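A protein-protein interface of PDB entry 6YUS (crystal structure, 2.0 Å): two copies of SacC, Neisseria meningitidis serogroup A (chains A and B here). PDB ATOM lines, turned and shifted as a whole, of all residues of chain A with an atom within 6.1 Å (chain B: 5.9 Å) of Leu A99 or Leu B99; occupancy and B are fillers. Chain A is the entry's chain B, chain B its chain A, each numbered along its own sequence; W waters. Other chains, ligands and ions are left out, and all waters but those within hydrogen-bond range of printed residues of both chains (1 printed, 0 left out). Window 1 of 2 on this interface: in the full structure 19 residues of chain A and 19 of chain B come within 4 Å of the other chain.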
ATOM      1  N   MET A   1      12.454  -4.661 -18.056  1.00  0.00           N
ATOM      2  CA  MET A   1      13.821  -5.117 -17.983  1.00  0.00           C
ATOM      3  C   MET A   1      14.056  -6.009 -19.193  1.00  0.00           C
ATOM      4  O   MET A   1      13.284  -6.897 -19.487  1.00  0.00           O
ATOM      5  CB  MET A   1      14.089  -5.853 -16.676  1.00  0.00           C
ATOM      6  CG  MET A   1      15.553  -6.244 -16.518  1.00  0.00           C
ATOM      7  SD  MET A   1      15.909  -6.893 -14.893  1.00  0.00           S
ATOM      8  CE  MET A   1      14.916  -8.357 -14.964  1.00  0.00           C
ATOM      9  N   LEU A   2      15.126  -5.703 -19.919  1.00  0.00           N
ATOM     10  CA  LEU A   2      15.400  -6.373 -21.177  1.00  0.00           C
ATOM     11  C   LEU A   2      15.287  -7.898 -21.058  1.00  0.00           C
ATOM     12  O   LEU A   2      14.632  -8.541 -21.885  1.00  0.00           O
ATOM     13  CB  LEU A   2      16.791  -5.956 -21.666  1.00  0.00           C
ATOM     14  CG  LEU A   2      17.283  -6.706 -22.891  1.00  0.00           C
ATOM     15  CD1 LEU A   2      16.289  -6.508 -24.022  1.00  0.00           C
ATOM     16  CD2 LEU A   2      18.655  -6.131 -23.271  1.00  0.00           C
ATOM     17  N   LEU A   5      11.981  -9.590 -21.369  1.00  0.00           N
ATOM     18  CA  LEU A   5      11.347  -9.609 -22.676  1.00  0.00           C
ATOM     19  C   LEU A   5      11.741 -10.826 -23.493  1.00  0.00           C
ATOM     20  O   LEU A   5      11.293 -10.957 -24.639  1.00  0.00           O
ATOM     21  CB  LEU A   5      11.719  -8.344 -23.448  1.00  0.00           C
ATOM     22  CG  LEU A   5      11.347  -7.062 -22.695  1.00  0.00           C
ATOM     23  CD1 LEU A   5      11.957  -5.900 -23.437  1.00  0.00           C
ATOM     24  CD2 LEU A   5       9.807  -6.944 -22.586  1.00  0.00           C
ATOM     25  N   LEU A  19       9.093  -7.012 -27.806  1.00  0.00           N
ATOM     26  CA  LEU A  19       8.565  -5.828 -27.139  1.00  0.00           C
ATOM     27  C   LEU A  19       7.483  -5.230 -28.016  1.00  0.00           C
ATOM     28  O   LEU A  19       7.748  -4.833 -29.151  1.00  0.00           O
ATOM     29  CB  LEU A  19       9.664  -4.798 -26.875  1.00  0.00           C
ATOM     30  CG  LEU A  19       9.163  -3.463 -26.289  1.00  0.00           C
ATOM     31  CD1 LEU A  19       8.627  -3.654 -24.905  1.00  0.00           C
ATOM     32  CD2 LEU A  19      10.321  -2.446 -26.272  1.00  0.00           C
ATOM     33  N   PHE A  24      13.211  -9.271 -31.768  1.00  0.00           N
ATOM     34  CA  PHE A  24      14.542  -8.837 -32.160  1.00  0.00           C
ATOM     35  C   PHE A  24      15.606  -9.644 -31.444  1.00  0.00           C
ATOM     36  O   PHE A  24      15.377 -10.216 -30.374  1.00  0.00           O
ATOM     37  CB  PHE A  24      14.773  -7.343 -31.879  1.00  0.00           C
ATOM     38  CG  PHE A  24      14.681  -6.952 -30.422  1.00  0.00           C
ATOM     39  CD1 PHE A  24      13.451  -6.713 -29.824  1.00  0.00           C
ATOM     40  CD2 PHE A  24      15.828  -6.771 -29.675  1.00  0.00           C
ATOM     41  CE1 PHE A  24      13.359  -6.288 -28.489  1.00  0.00           C
ATOM     42  CE2 PHE A  24      15.767  -6.353 -28.355  1.00  0.00           C
ATOM     43  CZ  PHE A  24      14.508  -6.116 -27.749  1.00  0.00           C
ATOM     44  N   HIS A  94      12.401   1.860 -33.384  1.00  0.00           N
ATOM     45  CA  HIS A  94      13.204   3.051 -33.111  1.00  0.00           C
ATOM     46  C   HIS A  94      13.538   3.165 -31.628  1.00  0.00           C
ATOM     47  O   HIS A  94      14.695   3.416 -31.259  1.00  0.00           O
ATOM     48  CB  HIS A  94      12.431   4.288 -33.603  1.00  0.00           C
ATOM     49  CG  HIS A  94      13.162   5.587 -33.413  1.00  0.00           C
ATOM     50  ND1 HIS A  94      14.465   5.773 -33.816  1.00  0.00           N
ATOM     51  CD2 HIS A  94      12.763   6.764 -32.875  1.00  0.00           C
ATOM     52  CE1 HIS A  94      14.840   7.009 -33.536  1.00  0.00           C
ATOM     53  NE2 HIS A  94      13.823   7.633 -32.965  1.00  0.00           N
ATOM     54  N   CYS A  95      12.531   2.996 -30.754  1.00  0.00           N
ATOM     55  CA  CYS A  95      12.790   3.051 -29.316  1.00  0.00           C
ATOM     56  C   CYS A  95      13.811   1.999 -28.913  1.00  0.00           C
ATOM     57  O   CYS A  95      14.706   2.247 -28.091  1.00  0.00           O
ATOM     58  CB  CYS A  95      11.477   2.844 -28.552  1.00  0.00           C
ATOM     59  SG  CYS A  95      10.268   4.186 -28.770  1.00  0.00           S
ATOM     60  N   ILE A  96      13.691   0.810 -29.489  1.00  0.00           N
ATOM     61  CA  ILE A  96      14.575  -0.285 -29.108  1.00  0.00           C
ATOM     62  C   ILE A  96      16.007   0.054 -29.502  1.00  0.00           C
ATOM     63  O   ILE A  96      16.938  -0.054 -28.691  1.00  0.00           O
ATOM     64  CB  ILE A  96      14.070  -1.588 -29.764  1.00  0.00           C
ATOM     65  CG1 ILE A  96      12.706  -1.993 -29.194  1.00  0.00           C
ATOM     66  CG2 ILE A  96      15.088  -2.715 -29.630  1.00  0.00           C
ATOM     67  CD1 ILE A  96      12.182  -3.225 -29.895  1.00  0.00           C
ATOM     68  N   ILE A  97      16.197   0.531 -30.746  1.00  0.00           N
ATOM     69  CA  ILE A  97      17.535   0.916 -31.209  1.00  0.00           C
ATOM     70  C   ILE A  97      18.061   2.057 -30.360  1.00  0.00           C
ATOM     71  O   ILE A  97      19.187   2.015 -29.861  1.00  0.00           O
ATOM     72  CB  ILE A  97      17.494   1.292 -32.701  1.00  0.00           C
ATOM     73  CG1 ILE A  97      17.121   0.075 -33.545  1.00  0.00           C
ATOM     74  CG2 ILE A  97      18.851   1.846 -33.163  1.00  0.00           C
ATOM     75  CD1 ILE A  97      16.817   0.417 -34.958  1.00  0.00           C
ATOM     76  N   GLN A  98      17.223   3.077 -30.132  1.00  0.00           N
ATOM     77  CA  GLN A  98      17.726   4.274 -29.462  1.00  0.00           C
ATOM     78  C   GLN A  98      18.132   4.003 -28.019  1.00  0.00           C
ATOM     79  O   GLN A  98      19.034   4.664 -27.508  1.00  0.00           O
ATOM     80  CB  GLN A  98      16.672   5.406 -29.486  1.00  0.00           C
ATOM     81  CG  GLN A  98      16.558   6.100 -30.835  1.00  0.00           C
ATOM     82  CD  GLN A  98      17.890   6.657 -31.297  1.00  0.00           C
ATOM     83  OE1 GLN A  98      18.500   7.441 -30.601  1.00  0.00           O
ATOM     84  NE2 GLN A  98      18.362   6.201 -32.444  1.00  0.00           N
ATOM     85  N   LEU A  99      17.521   3.017 -27.373  1.00  0.00           N
ATOM     86  CA  LEU A  99      17.768   2.810 -25.955  1.00  0.00           C
ATOM     87  C   LEU A  99      18.774   1.702 -25.660  1.00  0.00           C
ATOM     88  O   LEU A  99      19.358   1.711 -24.557  1.00  0.00           O
ATOM     89  CB  LEU A  99      16.446   2.497 -25.238  1.00  0.00           C
ATOM     90  CG  LEU A  99      15.460   3.662 -25.233  1.00  0.00           C
ATOM     91  CD1 LEU A  99      14.083   3.118 -24.866  1.00  0.00           C
ATOM     92  CD2 LEU A  99      15.863   4.746 -24.242  1.00  0.00           C
ATOM     93  N   LEU A 100      18.976   0.761 -26.606  1.00  0.00           N
ATOM     94  CA  LEU A 100      19.985  -0.297 -26.500  1.00  0.00           C
ATOM     95  C   LEU A 100      21.291  -0.021 -27.243  1.00  0.00           C
ATOM     96  O   LEU A 100      22.306  -0.640 -26.902  1.00  0.00           O
ATOM     97  CB  LEU A 100      19.434  -1.645 -27.020  1.00  0.00           C
ATOM     98  CG  LEU A 100      18.191  -2.220 -26.303  1.00  0.00           C
ATOM     99  CD1 LEU A 100      17.721  -3.525 -26.911  1.00  0.00           C
ATOM    100  CD2 LEU A 100      18.365  -2.372 -24.794  1.00  0.00           C
ATOM    101  N   SER A 101      21.292   0.827 -28.267  1.00  0.00           N
ATOM    102  CA  SER A 101      22.524   1.071 -28.988  1.00  0.00           C
ATOM    103  C   SER A 101      23.431   2.009 -28.216  1.00  0.00           C
ATOM    104  O   SER A 101      22.956   2.920 -27.535  1.00  0.00           O
ATOM    105  CB  SER A 101      22.217   1.683 -30.376  1.00  0.00           C
ATOM    106  OG  SER A 101      23.308   2.508 -30.797  1.00  0.00           O
ATOM    107  N   MET B   1      21.244   6.029 -28.882  1.00  0.00           N
ATOM    108  CA  MET B   1      21.971   6.059 -27.623  1.00  0.00           C
ATOM    109  C   MET B   1      21.313   7.017 -26.655  1.00  0.00           C
ATOM    110  O   MET B   1      21.017   8.151 -27.008  1.00  0.00           O
ATOM    111  CB  MET B   1      23.418   6.473 -27.865  1.00  0.00           C
ATOM    112  CG  MET B   1      24.302   6.493 -26.635  1.00  0.00           C
ATOM    113  SD  MET B   1      25.956   6.248 -27.257  1.00  0.00           S
ATOM    114  CE  MET B   1      26.018   7.639 -28.358  1.00  0.00           C
ATOM    115  N   LEU B   2      21.093   6.524 -25.437  1.00  0.00           N
ATOM    116  CA  LEU B   2      20.448   7.302 -24.381  1.00  0.00           C
ATOM    117  C   LEU B   2      21.118   8.664 -24.197  1.00  0.00           C
ATOM    118  O   LEU B   2      20.449   9.700 -24.186  1.00  0.00           O
ATOM    119  CB  LEU B   2      20.475   6.509 -23.079  1.00  0.00           C
ATOM    120  CG  LEU B   2      19.726   7.170 -21.924  1.00  0.00           C
ATOM    121  CD1 LEU B   2      18.252   7.331 -22.313  1.00  0.00           C
ATOM    122  CD2 LEU B   2      19.891   6.373 -20.636  1.00  0.00           C
ATOM    123  N   LEU B   5      19.968  11.290 -26.301  1.00  0.00           N
ATOM    124  CA  LEU B   5      18.599  11.758 -26.138  1.00  0.00           C
ATOM    125  C   LEU B   5      18.475  12.873 -25.109  1.00  0.00           C
ATOM    126  O   LEU B   5      17.363  13.352 -24.869  1.00  0.00           O
ATOM    127  CB  LEU B   5      17.674  10.614 -25.733  1.00  0.00           C
ATOM    128  CG  LEU B   5      17.650   9.377 -26.621  1.00  0.00           C
ATOM    129  CD1 LEU B   5      16.718   8.338 -26.030  1.00  0.00           C
ATOM    130  CD2 LEU B   5      17.222   9.768 -28.014  1.00  0.00           C
ATOM    131  N   LEU B  19      12.471  11.142 -26.112  1.00  0.00           N
ATOM    132  CA  LEU B  19      12.416  10.122 -27.157  1.00  0.00           C
ATOM    133  C   LEU B  19      11.012  10.125 -27.731  1.00  0.00           C
ATOM    134  O   LEU B  19      10.045   9.885 -27.001  1.00  0.00           O
ATOM    135  CB  LEU B  19      12.774   8.732 -26.622  1.00  0.00           C
ATOM    136  CG  LEU B  19      12.587   7.527 -27.574  1.00  0.00           C
ATOM    137  CD1 LEU B  19      13.639   7.546 -28.668  1.00  0.00           C
ATOM    138  CD2 LEU B  19      12.627   6.174 -26.857  1.00  0.00           C
ATOM    139  N   PHE B  24      11.401  12.697 -20.313  1.00  0.00           N
ATOM    140  CA  PHE B  24      11.452  11.887 -19.107  1.00  0.00           C
ATOM    141  C   PHE B  24      12.753  12.115 -18.351  1.00  0.00           C
ATOM    142  O   PHE B  24      13.781  12.476 -18.932  1.00  0.00           O
ATOM    143  CB  PHE B  24      11.244  10.378 -19.430  1.00  0.00           C
ATOM    144  CG  PHE B  24      12.354   9.727 -20.256  1.00  0.00           C
ATOM    145  CD1 PHE B  24      12.286   9.687 -21.646  1.00  0.00           C
ATOM    146  CD2 PHE B  24      13.412   9.096 -19.642  1.00  0.00           C
ATOM    147  CE1 PHE B  24      13.277   9.066 -22.413  1.00  0.00           C
ATOM    148  CE2 PHE B  24      14.436   8.443 -20.407  1.00  0.00           C
ATOM    149  CZ  PHE B  24      14.366   8.427 -21.794  1.00  0.00           C
ATOM    150  N   HIS B  94       6.073   2.872 -22.458  1.00  0.00           N
ATOM    151  CA  HIS B  94       6.271   1.452 -22.173  1.00  0.00           C
ATOM    152  C   HIS B  94       7.665   0.994 -22.586  1.00  0.00           C
ATOM    153  O   HIS B  94       8.392   0.354 -21.804  1.00  0.00           O
ATOM    154  CB  HIS B  94       5.179   0.644 -22.900  1.00  0.00           C
ATOM    155  CG  HIS B  94       5.192  -0.818 -22.598  1.00  0.00           C
ATOM    156  ND1 HIS B  94       5.243  -1.306 -21.309  1.00  0.00           N
ATOM    157  CD2 HIS B  94       5.167  -1.903 -23.414  1.00  0.00           C
ATOM    158  CE1 HIS B  94       5.223  -2.627 -21.339  1.00  0.00           C
ATOM    159  NE2 HIS B  94       5.174  -3.015 -22.603  1.00  0.00           N
ATOM    160  N   CYS B  95       8.063   1.310 -23.828  1.00  0.00           N
ATOM    161  CA  CYS B  95       9.383   0.890 -24.301  1.00  0.00           C
ATOM    162  C   CYS B  95      10.480   1.449 -23.417  1.00  0.00           C
ATOM    163  O   CYS B  95      11.443   0.750 -23.078  1.00  0.00           O
ATOM    164  CB  CYS B  95       9.618   1.339 -25.742  1.00  0.00           C
ATOM    165  SG  CYS B  95       8.502   0.548 -26.912  1.00  0.00           S
ATOM    166  N   ILE B  96      10.350   2.711 -23.030  1.00  0.00           N
ATOM    167  CA  ILE B  96      11.395   3.334 -22.238  1.00  0.00           C
ATOM    168  C   ILE B  96      11.545   2.593 -20.916  1.00  0.00           C
ATOM    169  O   ILE B  96      12.651   2.215 -20.528  1.00  0.00           O
ATOM    170  CB  ILE B  96      11.075   4.829 -22.032  1.00  0.00           C
ATOM    171  CG1 ILE B  96      11.183   5.585 -23.362  1.00  0.00           C
ATOM    172  CG2 ILE B  96      11.985   5.424 -20.976  1.00  0.00           C
ATOM    173  CD1 ILE B  96      10.350   6.894 -23.361  1.00  0.00           C
ATOM    174  N   ILE B  97      10.418   2.328 -20.240  1.00  0.00           N
ATOM    175  CA  ILE B  97      10.438   1.613 -18.964  1.00  0.00           C
ATOM    176  C   ILE B  97      10.977   0.206 -19.159  1.00  0.00           C
ATOM    177  O   ILE B  97      11.906  -0.232 -18.465  1.00  0.00           O
ATOM    178  CB  ILE B  97       9.027   1.592 -18.343  1.00  0.00           C
ATOM    179  CG1 ILE B  97       8.520   3.020 -18.052  1.00  0.00           C
ATOM    180  CG2 ILE B  97       9.022   0.777 -17.054  1.00  0.00           C
ATOM    181  CD1 ILE B  97       7.084   3.039 -17.503  1.00  0.00           C
ATOM    182  N   GLN B  98      10.448  -0.508 -20.154  1.00  0.00           N
ATOM    183  CA  GLN B  98      10.829  -1.907 -20.300  1.00  0.00           C
ATOM    184  C   GLN B  98      12.314  -2.047 -20.559  1.00  0.00           C
ATOM    185  O   GLN B  98      12.942  -3.007 -20.097  1.00  0.00           O
ATOM    186  CB  GLN B  98      10.032  -2.579 -21.420  1.00  0.00           C
ATOM    187  CG  GLN B  98       8.563  -2.884 -20.993  1.00  0.00           C
ATOM    188  CD  GLN B  98       8.486  -3.697 -19.733  1.00  0.00           C
ATOM    189  OE1 GLN B  98       9.023  -4.802 -19.667  1.00  0.00           O
ATOM    190  NE2 GLN B  98       7.836  -3.155 -18.717  1.00  0.00           N
ATOM    191  N   LEU B  99      12.901  -1.114 -21.304  1.00  0.00           N
ATOM    192  CA  LEU B  99      14.306  -1.306 -21.672  1.00  0.00           C
ATOM    193  C   LEU B  99      15.286  -0.684 -20.688  1.00  0.00           C
ATOM    194  O   LEU B  99      16.442  -1.122 -20.641  1.00  0.00           O
ATOM    195  CB  LEU B  99      14.582  -0.745 -23.066  1.00  0.00           C
ATOM    196  CG  LEU B  99      13.811  -1.460 -24.172  1.00  0.00           C
ATOM    197  CD1 LEU B  99      13.839  -0.671 -25.459  1.00  0.00           C
ATOM    198  CD2 LEU B  99      14.389  -2.840 -24.370  1.00  0.00           C
ATOM    199  N   LEU B 100      14.863   0.323 -19.921  1.00  0.00           N
ATOM    200  CA  LEU B 100      15.734   1.030 -18.987  1.00  0.00           C
ATOM    201  C   LEU B 100      15.633   0.514 -17.559  1.00  0.00           C
ATOM    202  O   LEU B 100      16.613   0.599 -16.816  1.00  0.00           O
ATOM    203  CB  LEU B 100      15.413   2.534 -18.988  1.00  0.00           C
ATOM    204  CG  LEU B 100      15.876   3.269 -20.256  1.00  0.00           C
ATOM    205  CD1 LEU B 100      15.658   4.799 -20.168  1.00  0.00           C
ATOM    206  CD2 LEU B 100      17.334   2.947 -20.571  1.00  0.00           C
ATOM    207  N   SER B 101      14.477   0.001 -17.152  1.00  0.00           N
ATOM    208  CA  SER B 101      14.325  -0.495 -15.792  1.00  0.00           C
ATOM    209  C   SER B 101      15.152  -1.767 -15.598  1.00  0.00           C
ATOM    210  O   SER B 101      15.414  -2.515 -16.543  1.00  0.00           O
ATOM    211  CB  SER B 101      12.840  -0.740 -15.482  1.00  0.00           C
ATOM    212  OG  SER B 101      12.713  -1.949 -14.753  1.00  0.00           O
HETATM  213  O   HOH W   1      16.654  -3.522 -19.104  1.00  0.00           O
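Leu A2 touches Gln B98, and with the chains exchanged Gln A98 touches Leu B2.
Leu A5 touches Gln B98, and with the chains exchanged Gln A98 touches Leu B5.
Leu A19 touches Gln B98, and with the chains exchanged Gln A98 touches Leu B19.
Ile A96 touches Leu B99, and with the chains exchanged Leu A99 touches Ile B96.
Positions printed for both chains: 1, 2, 5, 19, 24, 94, 95, 96, 97, 98, 99, 100 and 101.
Of the 18 pairs that touch across the chains among the printed residues, 16 have their exchanged pair printed and touching as well.
The backbone NH of Leu B2 is in hydrogen-bond range of the backbone carbonyl oxygen of Gln A98, 3.5 Å away.
The backbone NH (N) of Met B1 sits at hydrogen-bond distance from the backbone carbonyl oxygen (O) of Gln A98 (2.9 Å).
The backbone NH (N) of Leu A2 lies within hydrogen-bond range of the backbone carbonyl oxygen (O) of Gln B98 (3.5 Å).
The backbone carbonyl oxygen (O) of Gln B98 sits at hydrogen-bond distance from the backbone NH (N) of Met A1 (2.7 Å).
Printed residues of chain B within 4 Å of Leu A99: Leu B19, Cys B95, Ile B96 and Leu B99.
Of the printed residues of chain A, Leu B99 touches Ile A96 (3.7 Å) and Leu A99 (3.8 Å).
Printed residues of chain A within 4 Å of Leu B5: Gln A98 (3.7 Å).
Printed residues of chain B within 4 Å of Gln A98: Met B1, Leu B2, Leu B5 and Leu B19.
Of the printed residues of chain A, Ser B101 touches Met A1.
Ile A97 touches none of the printed residues of chain B.
Leu A100 touches none of the printed residues of chain B.
The nearest printed residue of chain B that does not touch Met A1 is Ile B97 (4.5 Å).
Water W1 lies within hydrogen-bond range of N of Leu A2 (2.8 Å), O of Leu B99 (2.9 Å) and O of Ser B101 (3.0 Å).
Ser B101 touches Met A1 (O to CA, 3.4 Å).
Cys B95 touches Leu A19 (SG to CD2, 3.6 Å).
CB of Gln B98 touches CD1 of Leu A19 (3.9 Å).
Cys A95 touches Leu B19 (SG to CD2, 3.6 Å).
Cys A95 touches Cys B95.
CD1 of Leu B99 touches CA of Ile A96, 3.7 Å away.
Leu B5 touches Gln A98.
Leu B19 touches Gln A98.
CD1 of Leu A99 touches CD1 of Leu B99, at 3.8 Å.
Met B1 touches Ser A101 (CA to O, 3.3 Å).
Hydrophobic or aromatic side chains of chain B that line the printed part of chain A: Met B1, Leu B5, Leu B19 and Leu B99.
Hydrophobic or aromatic side chains of chain A that line the printed part of chain B: Met A1, Leu A5, Leu A19 and Leu A99.
Along chain A the printed residues that touch a printed residue of chain B span positions 1 to 101.
Among the printed residues, 18 pairs touch across the chains.
Among the printed residues, no Asp or Glu carboxylate lies within 4 Å of a Lys or Arg side-chain nitrogen of the other chain.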
